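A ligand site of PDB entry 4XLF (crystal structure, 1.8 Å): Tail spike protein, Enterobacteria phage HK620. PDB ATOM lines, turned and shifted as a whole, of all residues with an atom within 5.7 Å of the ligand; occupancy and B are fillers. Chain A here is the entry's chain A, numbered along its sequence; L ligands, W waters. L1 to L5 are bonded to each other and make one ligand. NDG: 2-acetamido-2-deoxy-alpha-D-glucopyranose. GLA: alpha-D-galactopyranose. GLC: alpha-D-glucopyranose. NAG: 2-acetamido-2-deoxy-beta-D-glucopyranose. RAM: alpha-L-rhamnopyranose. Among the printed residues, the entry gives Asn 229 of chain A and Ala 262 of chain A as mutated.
NE2 of His 287 sits at hydrogen-bond distance from O4 of NDG L1. OD1 of Asn 205 sits at hydrogen-bond distance from O3 of NAG L4, 2.7 Å away. A ring nitrogen (ND1) of His 102 lies within hydrogen-bond range of an oxygen (O4) of RAM L5 (2.7 Å). The side-chain amide nitrogen (ND2) of Asn 236 lies within hydrogen-bond range of an oxygen (O4) of NAG L4 (2.7 Å). An oxygen (O2) of GLA L2 sits at hydrogen-bond distance from the side-chain hydroxyl (OH) of Tyr 234 (2.8 Å). ND2 of Asn 361 sits at hydrogen-bond distance from O4 of NDG L1, at 2.8 Å. An oxygen (O6) of NDG L1 sits at hydrogen-bond distance from a ring nitrogen (NE2) of His 264, at 2.9 Å. OE2 of Glu 290 sits at hydrogen-bond distance from N2 of NAG L4, at 2.9 Å. The indole nitrogen of Trp 198 is in hydrogen-bond range of an oxygen (O7) of NDG L1 (2.9 Å). ND2 of Asn 229 lies within hydrogen-bond range of O1 of NDG L1 (3.1 Å). O4 of RAM L5 sits at hydrogen-bond distance from NE2 of Gln 132 (3.1 Å).
Gly 101 touches the ligand. CZ of Phe 137 touches C6 of RAM L5, at 3.96 Å. Leu 172 touches the ligand. CG2 of Thr 197 touches O6 of GLA L2, 3.4 Å away. Thr 201 touches the ligand. Gly 203 touches the ligand. NE1 of Trp 204 touches O3 of NAG L4 (3.5 Å). His 230 touches the ligand. Ser 231 touches the ligand. CG of Tyr 283 touches O6 of NDG L1 (3.1 Å). Val 285 touches the ligand. CB of Ala 289 touches C8 of NAG L4 (3.96 Å). Hydrophobic or aromatic side chains within 4 Å of the ligand: His 102, Phe 137, Leu 172, Trp 198, Trp 204, Tyr 234, His 264, Tyr 283, Val 285, His 287 and Ala 289. Within 4 Å of the ligand: Gly 101, His 102, Gln 132, Phe 137, Leu 172, Thr 197, Trp 198, Thr 201, Gly 203, Trp 204, Asn 205, Asn 229, His 230, Ser 231, Tyr 234, Asn 236, His 264, Tyr 283, Val 285, His 287, Ala 289, Glu 290 and Asn 361. Along chain A the residues within 4 Å of the ligand span positions 101 to 361.
The backbone NH (N) of Asn 236 lies within hydrogen-bond range of the backbone carbonyl oxygen (O) of Leu 202, at 2.7 Å. OH of Tyr 234 lies close to ND1 of His 264. OE1 of Glu 290 sits at hydrogen-bond distance from ND1 of His 264 (2.7 Å). The side-chain amide oxygen (OD1) of Asn 174 sits close to the backbone carbonyl oxygen (O) of Trp 198, at 3.4 Å. The side-chain amide nitrogen (ND2) of Asn 174 is in hydrogen-bond range of the side-chain amide oxygen (OE1) of Gln 132 (3.2 Å). The backbone carbonyl oxygen (O) of Thr 197 is in hydrogen-bond range of the backbone NH (N) of Ser 231 (2.9 Å). The backbone carbonyl oxygen (O) of Thr 197 lies close to a ring nitrogen (ND1) of His 230 (3.3 Å). OG1 of Thr 201 lies within hydrogen-bond range of ND2 of Asn 174 (3.3 Å).
Water W15 bridges O3 of RAM L5 (2.6 Å) and O of Gly 101 (2.9 Å). Water W12 lies within hydrogen-bond range of an oxygen (O1) of NDG L1 (2.6 Å) and the side-chain hydroxyl (OH) of Tyr 283 (2.7 Å). Water W16 lies within hydrogen-bond range of the side-chain hydroxyl of Thr 201 and an oxygen (O6) of NAG L4. Water W6 bridges an oxygen (O2) of GLA L2 (2.9 Å) and the side-chain amide nitrogen of Asn 361 (3.5 Å). Water W13 lies within hydrogen-bond range of O3 of NAG L4 and NE1 of Trp 204. Water W10 lies within hydrogen-bond range of an oxygen (O3) of RAM L5, the side-chain hydroxyl of Ser 103 and the side-chain amide nitrogen of Gln 132.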
ATOM      1  N   GLY A 101      19.081  -0.583 -19.279  1.00  0.00           N
ATOM      2  CA  GLY A 101      17.759  -0.969 -19.768  1.00  0.00           C
ATOM      3  C   GLY A 101      16.650  -0.014 -19.313  1.00  0.00           C
ATOM      4  O   GLY A 101      15.529  -0.089 -19.825  1.00  0.00           O
ATOM      5  N   HIS A 102      16.933   0.867 -18.368  1.00  0.00           N
ATOM      6  CA  HIS A 102      15.983   1.810 -17.845  1.00  0.00           C
ATOM      7  C   HIS A 102      16.394   3.238 -18.157  1.00  0.00           C
ATOM      8  O   HIS A 102      15.893   4.160 -17.541  1.00  0.00           O
ATOM      9  CB  HIS A 102      15.874   1.651 -16.344  1.00  0.00           C
ATOM     10  CG  HIS A 102      15.628   0.251 -15.898  1.00  0.00           C
ATOM     11  ND1 HIS A 102      14.376  -0.222 -15.625  1.00  0.00           N
ATOM     12  CD2 HIS A 102      16.474  -0.742 -15.611  1.00  0.00           C
ATOM     13  CE1 HIS A 102      14.448  -1.449 -15.158  1.00  0.00           C
ATOM     14  NE2 HIS A 102      15.725  -1.809 -15.169  1.00  0.00           N
ATOM     15  N   SER A 103      17.249   3.406 -19.173  1.00  0.00           N
ATOM     16  CA  SER A 103      17.794   4.779 -19.502  1.00  0.00           C
ATOM     17  C   SER A 103      18.341   5.443 -18.254  1.00  0.00           C
ATOM     18  O   SER A 103      18.280   6.648 -18.133  1.00  0.00           O
ATOM     19  CB  SER A 103      16.746   5.652 -20.135  1.00  0.00           C
ATOM     20  OG  SER A 103      16.084   4.939 -21.169  1.00  0.00           O
ATOM     21  N   GLN A 132      16.241   8.141 -16.647  1.00  0.00           N
ATOM     22  CA  GLN A 132      15.738   7.929 -15.287  1.00  0.00           C
ATOM     23  C   GLN A 132      16.866   8.175 -14.405  1.00  0.00           C
ATOM     24  O   GLN A 132      17.896   7.462 -14.450  1.00  0.00           O
ATOM     25  CB  GLN A 132      15.221   6.527 -15.115  1.00  0.00           C
ATOM     26  CG  GLN A 132      13.972   6.277 -15.971  1.00  0.00           C
ATOM     27  CD  GLN A 132      13.227   5.004 -15.563  1.00  0.00           C
ATOM     28  OE1 GLN A 132      12.738   4.846 -14.411  1.00  0.00           O
ATOM     29  NE2 GLN A 132      13.024   4.135 -16.527  1.00  0.00           N
ATOM     30  N   PHE A 137      16.870  -0.601  -9.678  1.00  0.00           N
ATOM     31  CA  PHE A 137      16.984  -1.903 -10.320  1.00  0.00           C
ATOM     32  C   PHE A 137      18.476  -2.212 -10.570  1.00  0.00           C
ATOM     33  O   PHE A 137      19.258  -1.308 -10.808  1.00  0.00           O
ATOM     34  CB  PHE A 137      16.227  -1.914 -11.652  1.00  0.00           C
ATOM     35  CG  PHE A 137      14.709  -1.758 -11.544  1.00  0.00           C
ATOM     36  CD1 PHE A 137      13.916  -2.787 -11.027  1.00  0.00           C
ATOM     37  CD2 PHE A 137      14.114  -0.648 -12.047  1.00  0.00           C
ATOM     38  CE1 PHE A 137      12.520  -2.613 -10.997  1.00  0.00           C
ATOM     39  CE2 PHE A 137      12.760  -0.469 -12.077  1.00  0.00           C
ATOM     40  CZ  PHE A 137      11.955  -1.478 -11.553  1.00  0.00           C
ATOM     41  N   PRO A 142      13.249  -5.976 -14.997  1.00  0.00           N
ATOM     42  CA  PRO A 142      12.873  -5.849 -13.586  1.00  0.00           C
ATOM     43  C   PRO A 142      12.535  -7.177 -12.931  1.00  0.00           C
ATOM     44  O   PRO A 142      12.799  -7.382 -11.712  1.00  0.00           O
ATOM     45  CB  PRO A 142      11.679  -4.881 -13.601  1.00  0.00           C
ATOM     46  CG  PRO A 142      11.263  -4.710 -15.003  1.00  0.00           C
ATOM     47  CD  PRO A 142      12.432  -5.132 -15.879  1.00  0.00           C
ATOM     48  N   LEU A 172      10.209   7.545 -21.967  1.00  0.00           N
ATOM     49  CA  LEU A 172       9.924   7.634 -20.497  1.00  0.00           C
ATOM     50  C   LEU A 172      11.032   8.450 -19.801  1.00  0.00           C
ATOM     51  O   LEU A 172      12.241   8.385 -20.146  1.00  0.00           O
ATOM     52  CB  LEU A 172       9.800   6.241 -19.824  1.00  0.00           C
ATOM     53  CG  LEU A 172       8.802   5.249 -20.452  1.00  0.00           C
ATOM     54  CD1 LEU A 172       9.062   3.793 -20.038  1.00  0.00           C
ATOM     55  CD2 LEU A 172       7.393   5.656 -20.181  1.00  0.00           C
ATOM     56  N   ASN A 174      12.022   9.784 -15.635  1.00  0.00           N
ATOM     57  CA  ASN A 174      11.776   9.590 -14.186  1.00  0.00           C
ATOM     58  C   ASN A 174      12.909  10.302 -13.445  1.00  0.00           C
ATOM     59  O   ASN A 174      14.012  10.418 -13.970  1.00  0.00           O
ATOM     60  CB  ASN A 174      11.751   8.086 -13.858  1.00  0.00           C
ATOM     61  CG  ASN A 174      11.136   7.738 -12.486  1.00  0.00           C
ATOM     62  OD1 ASN A 174      10.596   8.566 -11.719  1.00  0.00           O
ATOM     63  ND2 ASN A 174      11.140   6.431 -12.203  1.00  0.00           N
ATOM     64  N   THR A 197       7.744  11.740 -17.089  1.00  0.00           N
ATOM     65  CA  THR A 197       6.633  10.887 -17.003  1.00  0.00           C
ATOM     66  C   THR A 197       6.219  10.772 -15.491  1.00  0.00           C
ATOM     67  O   THR A 197       5.031  10.821 -15.123  1.00  0.00           O
ATOM     68  CB  THR A 197       6.999   9.490 -17.491  1.00  0.00           C
ATOM     69  OG1 THR A 197       7.552   9.526 -18.825  1.00  0.00           O
ATOM     70  CG2 THR A 197       5.769   8.619 -17.407  1.00  0.00           C
ATOM     71  N   TRP A 198       7.216  10.588 -14.668  1.00  0.00           N
ATOM     72  CA  TRP A 198       7.091  10.508 -13.169  1.00  0.00           C
ATOM     73  C   TRP A 198       8.286  11.277 -12.564  1.00  0.00           C
ATOM     74  O   TRP A 198       9.362  11.403 -13.233  1.00  0.00           O
ATOM     75  CB  TRP A 198       7.185   9.087 -12.655  1.00  0.00           C
ATOM     76  CG  TRP A 198       6.432   8.058 -13.359  1.00  0.00           C
ATOM     77  CD1 TRP A 198       5.112   7.810 -13.270  1.00  0.00           C
ATOM     78  CD2 TRP A 198       6.986   7.098 -14.290  1.00  0.00           C
ATOM     79  NE1 TRP A 198       4.797   6.714 -14.068  1.00  0.00           N
ATOM     80  CE2 TRP A 198       5.918   6.316 -14.746  1.00  0.00           C
ATOM     81  CE3 TRP A 198       8.270   6.866 -14.781  1.00  0.00           C
ATOM     82  CZ2 TRP A 198       6.106   5.271 -15.691  1.00  0.00           C
ATOM     83  CZ3 TRP A 198       8.455   5.878 -15.744  1.00  0.00           C
ATOM     84  CH2 TRP A 198       7.367   5.072 -16.148  1.00  0.00           C
ATOM     85  N   THR A 201       9.127   6.859  -8.567  1.00  0.00           N
ATOM     86  CA  THR A 201       8.350   5.651  -8.491  1.00  0.00           C
ATOM     87  C   THR A 201       8.837   4.692  -7.416  1.00  0.00           C
ATOM     88  O   THR A 201      10.045   4.628  -7.146  1.00  0.00           O
ATOM     89  CB  THR A 201       8.394   4.852  -9.798  1.00  0.00           C
ATOM     90  OG1 THR A 201       9.717   4.362 -10.042  1.00  0.00           O
ATOM     91  CG2 THR A 201       7.906   5.711 -10.940  1.00  0.00           C
ATOM     92  N   LEU A 202       7.883   4.055  -6.766  1.00  0.00           N
ATOM     93  CA  LEU A 202       8.158   3.245  -5.619  1.00  0.00           C
ATOM     94  C   LEU A 202       7.728   1.846  -5.988  1.00  0.00           C
ATOM     95  O   LEU A 202       6.583   1.637  -6.432  1.00  0.00           O
ATOM     96  CB  LEU A 202       7.348   3.681  -4.418  1.00  0.00           C
ATOM     97  CG  LEU A 202       7.422   5.142  -4.031  1.00  0.00           C
ATOM     98  CD1 LEU A 202       6.512   5.430  -2.835  1.00  0.00           C
ATOM     99  CD2 LEU A 202       8.849   5.602  -3.790  1.00  0.00           C
ATOM    100  N   GLY A 203       8.624   0.921  -5.819  1.00  0.00           N
ATOM    101  CA  GLY A 203       8.250  -0.502  -6.011  1.00  0.00           C
ATOM    102  C   GLY A 203       8.172  -0.892  -7.457  1.00  0.00           C
ATOM    103  O   GLY A 203       8.340  -0.072  -8.355  1.00  0.00           O
ATOM    104  N   TRP A 204       7.880  -2.163  -7.686  1.00  0.00           N
ATOM    105  CA  TRP A 204       7.730  -2.724  -9.021  1.00  0.00           C
ATOM    106  C   TRP A 204       6.737  -3.847  -8.965  1.00  0.00           C
ATOM    107  O   TRP A 204       7.026  -4.905  -8.390  1.00  0.00           O
ATOM    108  CB  TRP A 204       9.044  -3.178  -9.674  1.00  0.00           C
ATOM    109  CG  TRP A 204       8.805  -3.767 -11.020  1.00  0.00           C
ATOM    110  CD1 TRP A 204       8.468  -3.088 -12.143  1.00  0.00           C
ATOM    111  CD2 TRP A 204       8.744  -5.157 -11.335  1.00  0.00           C
ATOM    112  NE1 TRP A 204       8.228  -3.969 -13.178  1.00  0.00           N
ATOM    113  CE2 TRP A 204       8.395  -5.252 -12.719  1.00  0.00           C
ATOM    114  CE3 TRP A 204       8.955  -6.332 -10.616  1.00  0.00           C
ATOM    115  CZ2 TRP A 204       8.272  -6.446 -13.355  1.00  0.00           C
ATOM    116  CZ3 TRP A 204       8.843  -7.535 -11.250  1.00  0.00           C
ATOM    117  CH2 TRP A 204       8.502  -7.598 -12.629  1.00  0.00           C
ATOM    118  N   ASN A 205       5.579  -3.604  -9.580  1.00  0.00           N
ATOM    119  CA  ASN A 205       4.503  -4.578  -9.729  1.00  0.00           C
ATOM    120  C   ASN A 205       4.231  -5.367  -8.486  1.00  0.00           C
ATOM    121  O   ASN A 205       4.160  -6.579  -8.522  1.00  0.00           O
ATOM    122  CB  ASN A 205       4.741  -5.490 -10.912  1.00  0.00           C
ATOM    123  CG  ASN A 205       4.650  -4.794 -12.239  1.00  0.00           C
ATOM    124  OD1 ASN A 205       4.385  -3.578 -12.329  1.00  0.00           O
ATOM    125  ND2 ASN A 205       4.964  -5.544 -13.298  1.00  0.00           N
ATOM    126  N   ASN A 229       1.838  11.528 -20.880  1.00  0.00           N
ATOM    127  CA  ASN A 229       1.182  11.101 -19.630  1.00  0.00           C
ATOM    128  C   ASN A 229       2.121  11.365 -18.525  1.00  0.00           C
ATOM    129  O   ASN A 229       3.350  11.195 -18.684  1.00  0.00           O
ATOM    130  CB  ASN A 229       0.859   9.607 -19.699  1.00  0.00           C
ATOM    131  CG  ASN A 229      -0.258   9.180 -18.771  1.00  0.00           C
ATOM    132  OD1 ASN A 229      -0.563   9.806 -17.735  1.00  0.00           O
ATOM    133  ND2 ASN A 229      -0.857   8.066 -19.124  1.00  0.00           N
ATOM    134  N   HIS A 230       1.565  11.796 -17.404  1.00  0.00           N
ATOM    135  CA  HIS A 230       2.370  12.091 -16.238  1.00  0.00           C
ATOM    136  C   HIS A 230       1.676  11.758 -14.941  1.00  0.00           C
ATOM    137  O   HIS A 230       0.499  12.078 -14.820  1.00  0.00           O
ATOM    138  CB  HIS A 230       2.716  13.561 -16.205  1.00  0.00           C
ATOM    139  CG  HIS A 230       3.481  13.973 -14.976  1.00  0.00           C
ATOM    140  ND1 HIS A 230       4.852  14.157 -14.963  1.00  0.00           N
ATOM    141  CD2 HIS A 230       3.048  14.296 -13.734  1.00  0.00           C
ATOM    142  CE1 HIS A 230       5.218  14.561 -13.770  1.00  0.00           C
ATOM    143  NE2 HIS A 230       4.144  14.660 -13.009  1.00  0.00           N
ATOM    144  N   SER A 231       2.383  11.069 -14.064  1.00  0.00           N
ATOM    145  CA  SER A 231       1.972  10.808 -12.654  1.00  0.00           C
ATOM    146  C   SER A 231       3.187  11.101 -11.764  1.00  0.00           C
ATOM    147  O   SER A 231       4.195  10.440 -11.867  1.00  0.00           O
ATOM    148  CB  SER A 231       1.473   9.395 -12.418  1.00  0.00           C
ATOM    149  OG  SER A 231       0.984   9.311 -11.095  1.00  0.00           O
ATOM    150  N   TYR A 234       4.358   7.403  -8.504  1.00  0.00           N
ATOM    151  CA  TYR A 234       3.663   6.151  -8.711  1.00  0.00           C
ATOM    152  C   TYR A 234       4.013   5.126  -7.613  1.00  0.00           C
ATOM    153  O   TYR A 234       5.181   4.796  -7.430  1.00  0.00           O
ATOM    154  CB  TYR A 234       4.013   5.632 -10.102  1.00  0.00           C
ATOM    155  CG  TYR A 234       3.118   4.634 -10.816  1.00  0.00           C
ATOM    156  CD1 TYR A 234       3.039   3.308 -10.423  1.00  0.00           C
ATOM    157  CD2 TYR A 234       2.431   4.994 -11.972  1.00  0.00           C
ATOM    158  CE1 TYR A 234       2.239   2.387 -11.132  1.00  0.00           C
ATOM    159  CE2 TYR A 234       1.661   4.068 -12.659  1.00  0.00           C
ATOM    160  CZ  TYR A 234       1.581   2.771 -12.270  1.00  0.00           C
ATOM    161  OH  TYR A 234       0.863   1.841 -13.016  1.00  0.00           O
ATOM    162  N   ASN A 236       3.857   1.586  -6.357  1.00  0.00           N
ATOM    163  CA  ASN A 236       3.649   0.251  -6.876  1.00  0.00           C
ATOM    164  C   ASN A 236       4.198  -0.835  -5.944  1.00  0.00           C
ATOM    165  O   ASN A 236       4.581  -1.899  -6.363  1.00  0.00           O
ATOM    166  CB  ASN A 236       4.273   0.133  -8.258  1.00  0.00           C
ATOM    167  CG  ASN A 236       3.524  -0.852  -9.169  1.00  0.00           C
ATOM    168  OD1 ASN A 236       2.567  -1.461  -8.766  1.00  0.00           O
ATOM    169  ND2 ASN A 236       4.036  -1.005 -10.390  1.00  0.00           N
ATOM    170  N   ALA A 262      -0.359   8.048  -8.078  1.00  0.00           N
ATOM    171  CA  ALA A 262      -1.053   6.833  -8.391  1.00  0.00           C
ATOM    172  C   ALA A 262      -0.851   5.872  -7.206  1.00  0.00           C
ATOM    173  O   ALA A 262       0.287   5.493  -6.918  1.00  0.00           O
ATOM    174  CB  ALA A 262      -0.508   6.181  -9.656  1.00  0.00           C
ATOM    175  N   HIS A 264      -1.314   2.128  -6.279  1.00  0.00           N
ATOM    176  CA  HIS A 264      -1.583   0.928  -7.041  1.00  0.00           C
ATOM    177  C   HIS A 264      -1.350  -0.409  -6.341  1.00  0.00           C
ATOM    178  O   HIS A 264      -1.351  -1.459  -7.011  1.00  0.00           O
ATOM    179  CB  HIS A 264      -0.759   0.953  -8.353  1.00  0.00           C
ATOM    180  CG  HIS A 264      -1.363   1.737  -9.480  1.00  0.00           C
ATOM    181  ND1 HIS A 264      -1.175   1.361 -10.786  1.00  0.00           N
ATOM    182  CD2 HIS A 264      -2.114   2.848  -9.527  1.00  0.00           C
ATOM    183  CE1 HIS A 264      -1.784   2.206 -11.599  1.00  0.00           C
ATOM    184  NE2 HIS A 264      -2.301   3.163 -10.868  1.00  0.00           N
ATOM    185  N   TYR A 283      -4.920   8.584  -8.842  1.00  0.00           N
ATOM    186  CA  TYR A 283      -5.485   7.275  -9.239  1.00  0.00           C
ATOM    187  C   TYR A 283      -5.400   6.267  -8.043  1.00  0.00           C
ATOM    188  O   TYR A 283      -4.393   6.165  -7.372  1.00  0.00           O
ATOM    189  CB  TYR A 283      -4.773   6.648 -10.459  1.00  0.00           C
ATOM    190  CG  TYR A 283      -5.086   7.357 -11.747  1.00  0.00           C
ATOM    191  CD1 TYR A 283      -6.200   6.987 -12.501  1.00  0.00           C
ATOM    192  CD2 TYR A 283      -4.294   8.400 -12.234  1.00  0.00           C
ATOM    193  CE1 TYR A 283      -6.502   7.628 -13.698  1.00  0.00           C
ATOM    194  CE2 TYR A 283      -4.595   9.003 -13.406  1.00  0.00           C
ATOM    195  CZ  TYR A 283      -5.690   8.628 -14.139  1.00  0.00           C
ATOM    196  OH  TYR A 283      -5.984   9.292 -15.309  1.00  0.00           O
ATOM    197  N   VAL A 285      -6.059   2.314  -8.066  1.00  0.00           N
ATOM    198  CA  VAL A 285      -6.333   1.364  -9.153  1.00  0.00           C
ATOM    199  C   VAL A 285      -5.611   0.086  -8.824  1.00  0.00           C
ATOM    200  O   VAL A 285      -4.467   0.130  -8.328  1.00  0.00           O
ATOM    201  CB  VAL A 285      -5.834   1.942 -10.491  1.00  0.00           C
ATOM    202  CG1 VAL A 285      -5.949   0.882 -11.638  1.00  0.00           C
ATOM    203  CG2 VAL A 285      -6.623   3.197 -10.880  1.00  0.00           C
ATOM    204  N   HIS A 287      -4.263  -2.669 -11.202  1.00  0.00           N
ATOM    205  CA  HIS A 287      -3.991  -3.263 -12.516  1.00  0.00           C
ATOM    206  C   HIS A 287      -3.620  -4.755 -12.355  1.00  0.00           C
ATOM    207  O   HIS A 287      -2.618  -5.107 -11.651  1.00  0.00           O
ATOM    208  CB  HIS A 287      -2.808  -2.604 -13.179  1.00  0.00           C
ATOM    209  CG  HIS A 287      -3.065  -1.252 -13.762  1.00  0.00           C
ATOM    210  ND1 HIS A 287      -4.221  -0.880 -14.393  1.00  0.00           N
ATOM    211  CD2 HIS A 287      -2.250  -0.163 -13.840  1.00  0.00           C
ATOM    212  CE1 HIS A 287      -4.126   0.362 -14.825  1.00  0.00           C
ATOM    213  NE2 HIS A 287      -2.956   0.846 -14.447  1.00  0.00           N
ATOM    214  N   ALA A 289      -2.164  -6.391 -14.422  1.00  0.00           N
ATOM    215  CA  ALA A 289      -0.791  -6.443 -14.893  1.00  0.00           C
ATOM    216  C   ALA A 289       0.290  -6.163 -13.885  1.00  0.00           C
ATOM    217  O   ALA A 289       1.478  -6.394 -14.179  1.00  0.00           O
ATOM    218  CB  ALA A 289      -0.635  -5.459 -16.065  1.00  0.00           C
ATOM    219  N   GLU A 290      -0.065  -5.595 -12.733  1.00  0.00           N
ATOM    220  CA  GLU A 290       0.871  -5.225 -11.743  1.00  0.00           C
ATOM    221  C   GLU A 290       0.725  -6.087 -10.495  1.00  0.00           C
ATOM    222  O   GLU A 290       1.219  -5.738  -9.461  1.00  0.00           O
ATOM    223  CB  GLU A 290       0.673  -3.715 -11.395  1.00  0.00           C
ATOM    224  CG  GLU A 290       0.957  -2.828 -12.600  1.00  0.00           C
ATOM    225  CD  GLU A 290       0.853  -1.358 -12.293  1.00  0.00           C
ATOM    226  OE1 GLU A 290       0.077  -0.988 -11.374  1.00  0.00           O
ATOM    227  OE2 GLU A 290       1.506  -0.560 -12.966  1.00  0.00           O
ATOM    228  N   ASN A 361      -7.702   1.042 -19.252  1.00  0.00           N
ATOM    229  CA  ASN A 361      -6.914   1.776 -20.235  1.00  0.00           C
ATOM    230  C   ASN A 361      -7.321   1.526 -21.693  1.00  0.00           C
ATOM    231  O   ASN A 361      -7.056   2.352 -22.507  1.00  0.00           O
ATOM    232  CB  ASN A 361      -5.392   1.546 -20.061  1.00  0.00           C
ATOM    233  CG  ASN A 361      -4.855   2.238 -18.827  1.00  0.00           C
ATOM    234  OD1 ASN A 361      -5.539   3.064 -18.247  1.00  0.00           O
ATOM    235  ND2 ASN A 361      -3.634   1.902 -18.409  1.00  0.00           N
HETATM  236  C1  NDG L   1      -2.105   6.965 -15.316  1.00  0.00           C
HETATM  237  C2  NDG L   1      -0.781   6.196 -15.382  1.00  0.00           C
HETATM  238  C3  NDG L   1      -0.992   4.863 -16.114  1.00  0.00           C
HETATM  239  C4  NDG L   1      -2.120   4.086 -15.373  1.00  0.00           C
HETATM  240  C5  NDG L   1      -3.434   4.926 -15.164  1.00  0.00           C
HETATM  241  C6  NDG L   1      -4.361   4.288 -14.079  1.00  0.00           C
HETATM  242  C7  NDG L   1       1.447   7.204 -15.564  1.00  0.00           C
HETATM  243  C8  NDG L   1       2.278   8.210 -16.267  1.00  0.00           C
HETATM  244  O5  NDG L   1      -3.122   6.232 -14.677  1.00  0.00           O
HETATM  245  O3  NDG L   1       0.212   4.080 -16.153  1.00  0.00           O
HETATM  246  O4  NDG L   1      -2.462   2.859 -16.013  1.00  0.00           O
HETATM  247  O6  NDG L   1      -3.740   4.710 -12.786  1.00  0.00           O
HETATM  248  O7  NDG L   1       1.913   6.486 -14.642  1.00  0.00           O
HETATM  249  N2  NDG L   1       0.174   7.101 -15.997  1.00  0.00           N
HETATM  250  O1  NDG L   1      -2.504   7.284 -16.606  1.00  0.00           O
HETATM  251  C1  GLA L   2       0.322   3.282 -17.336  1.00  0.00           C
HETATM  252  C2  GLA L   2       1.274   2.149 -16.935  1.00  0.00           C
HETATM  253  C3  GLA L   2       2.680   2.715 -16.578  1.00  0.00           C
HETATM  254  C4  GLA L   2       3.199   3.620 -17.675  1.00  0.00           C
HETATM  255  C5  GLA L   2       2.157   4.712 -17.962  1.00  0.00           C
HETATM  256  C6  GLA L   2       2.505   5.651 -19.101  1.00  0.00           C
HETATM  257  O2  GLA L   2       0.729   1.469 -15.809  1.00  0.00           O
HETATM  258  O3  GLA L   2       3.528   1.587 -16.395  1.00  0.00           O
HETATM  259  O4  GLA L   2       3.409   2.852 -18.897  1.00  0.00           O
HETATM  260  O5  GLA L   2       0.895   4.094 -18.317  1.00  0.00           O
HETATM  261  O6  GLA L   2       3.771   6.273 -18.868  1.00  0.00           O
HETATM  262  C1  GLC L   3       4.707   3.085 -19.470  1.00  0.00           C
HETATM  263  C2  GLC L   3       4.755   2.427 -20.855  1.00  0.00           C
HETATM  264  C3  GLC L   3       4.720   0.882 -20.755  1.00  0.00           C
HETATM  265  C4  GLC L   3       5.891   0.469 -19.905  1.00  0.00           C
HETATM  266  C5  GLC L   3       5.753   1.124 -18.502  1.00  0.00           C
HETATM  267  C6  GLC L   3       6.873   0.808 -17.506  1.00  0.00           C
HETATM  268  O2  GLC L   3       3.628   2.867 -21.596  1.00  0.00           O
HETATM  269  O3  GLC L   3       4.884   0.410 -22.089  1.00  0.00           O
HETATM  270  O4  GLC L   3       5.876  -0.921 -19.793  1.00  0.00           O
HETATM  271  O5  GLC L   3       5.757   2.566 -18.682  1.00  0.00           O
HETATM  272  O6  GLC L   3       8.134   1.173 -18.137  1.00  0.00           O
HETATM  273  C1  NAG L   4       3.877   1.369 -15.009  1.00  0.00           C
HETATM  274  C2  NAG L   4       4.321  -0.108 -14.988  1.00  0.00           C
HETATM  275  C3  NAG L   4       4.901  -0.467 -13.625  1.00  0.00           C
HETATM  276  C4  NAG L   4       5.837   0.578 -13.027  1.00  0.00           C
HETATM  277  C5  NAG L   4       5.204   1.908 -13.157  1.00  0.00           C
HETATM  278  C6  NAG L   4       6.103   3.016 -12.751  1.00  0.00           C
HETATM  279  C7  NAG L   4       3.041  -1.650 -16.353  1.00  0.00           C
HETATM  280  C8  NAG L   4       1.729  -2.326 -16.591  1.00  0.00           C
HETATM  281  N2  NAG L   4       3.126  -0.858 -15.303  1.00  0.00           N
HETATM  282  O3  NAG L   4       5.576  -1.700 -13.778  1.00  0.00           O
HETATM  283  O4  NAG L   4       6.089   0.287 -11.615  1.00  0.00           O
HETATM  284  O5  NAG L   4       4.921   2.177 -14.496  1.00  0.00           O
HETATM  285  O6  NAG L   4       7.306   3.072 -13.475  1.00  0.00           O
HETATM  286  O7  NAG L   4       4.002  -1.865 -17.102  1.00  0.00           O
HETATM  287  C1  RAM L   5       8.908  -0.036 -18.300  1.00  0.00           C
HETATM  288  C2  RAM L   5      10.198   0.382 -18.998  1.00  0.00           C
HETATM  289  C3  RAM L   5      11.092   1.126 -18.069  1.00  0.00           C
HETATM  290  C4  RAM L   5      11.266   0.384 -16.743  1.00  0.00           C
HETATM  291  C5  RAM L   5       9.910   0.118 -16.159  1.00  0.00           C
HETATM  292  C6  RAM L   5       9.988  -0.803 -14.924  1.00  0.00           C
HETATM  293  O2  RAM L   5      10.850  -0.819 -19.428  1.00  0.00           O
HETATM  294  O3  RAM L   5      12.362   1.210 -18.754  1.00  0.00           O
HETATM  295  O4  RAM L   5      12.119   1.193 -15.905  1.00  0.00           O
HETATM  296  O5  RAM L   5       9.160  -0.697 -17.082  1.00  0.00           O
HETATM  297  O   HOH W   1       6.204   2.498  -9.347  1.00  0.00           O
HETATM  298  O   HOH W   2       5.038  -4.485 -16.069  1.00  0.00           O
HETATM  299  O   HOH W   3       8.658   0.136 -11.095  1.00  0.00           O
HETATM  300  O   HOH W   4       3.407   1.041 -24.121  1.00  0.00           O
HETATM  301  O   HOH W   5       4.268  -2.289 -22.799  1.00  0.00           O
HETATM  302  O   HOH W   6      -1.101  -0.193 -17.292  1.00  0.00           O
HETATM  303  O   HOH W   7       5.607   4.283 -23.527  1.00  0.00           O
HETATM  304  O   HOH W   8       6.457   0.988 -24.058  1.00  0.00           O
HETATM  305  O   HOH W   9      11.770   2.487 -13.637  1.00  0.00           O
HETATM  306  O   HOH W  10      13.191   3.930 -19.945  1.00  0.00           O
HETATM  307  O   HOH W  11       1.021   2.601 -20.771  1.00  0.00           O
HETATM  308  O   HOH W  12      -4.116   9.282 -17.198  1.00  0.00           O
HETATM  309  O   HOH W  13       7.383  -2.876 -15.809  1.00  0.00           O
HETATM  310  O   HOH W  14       4.155   8.009 -20.796  1.00  0.00           O
HETATM  311  O   HOH W  15      13.196   0.883 -21.190  1.00  0.00           O
HETATM  312  O   HOH W  16       9.644   2.648 -12.091  1.00  0.00           O
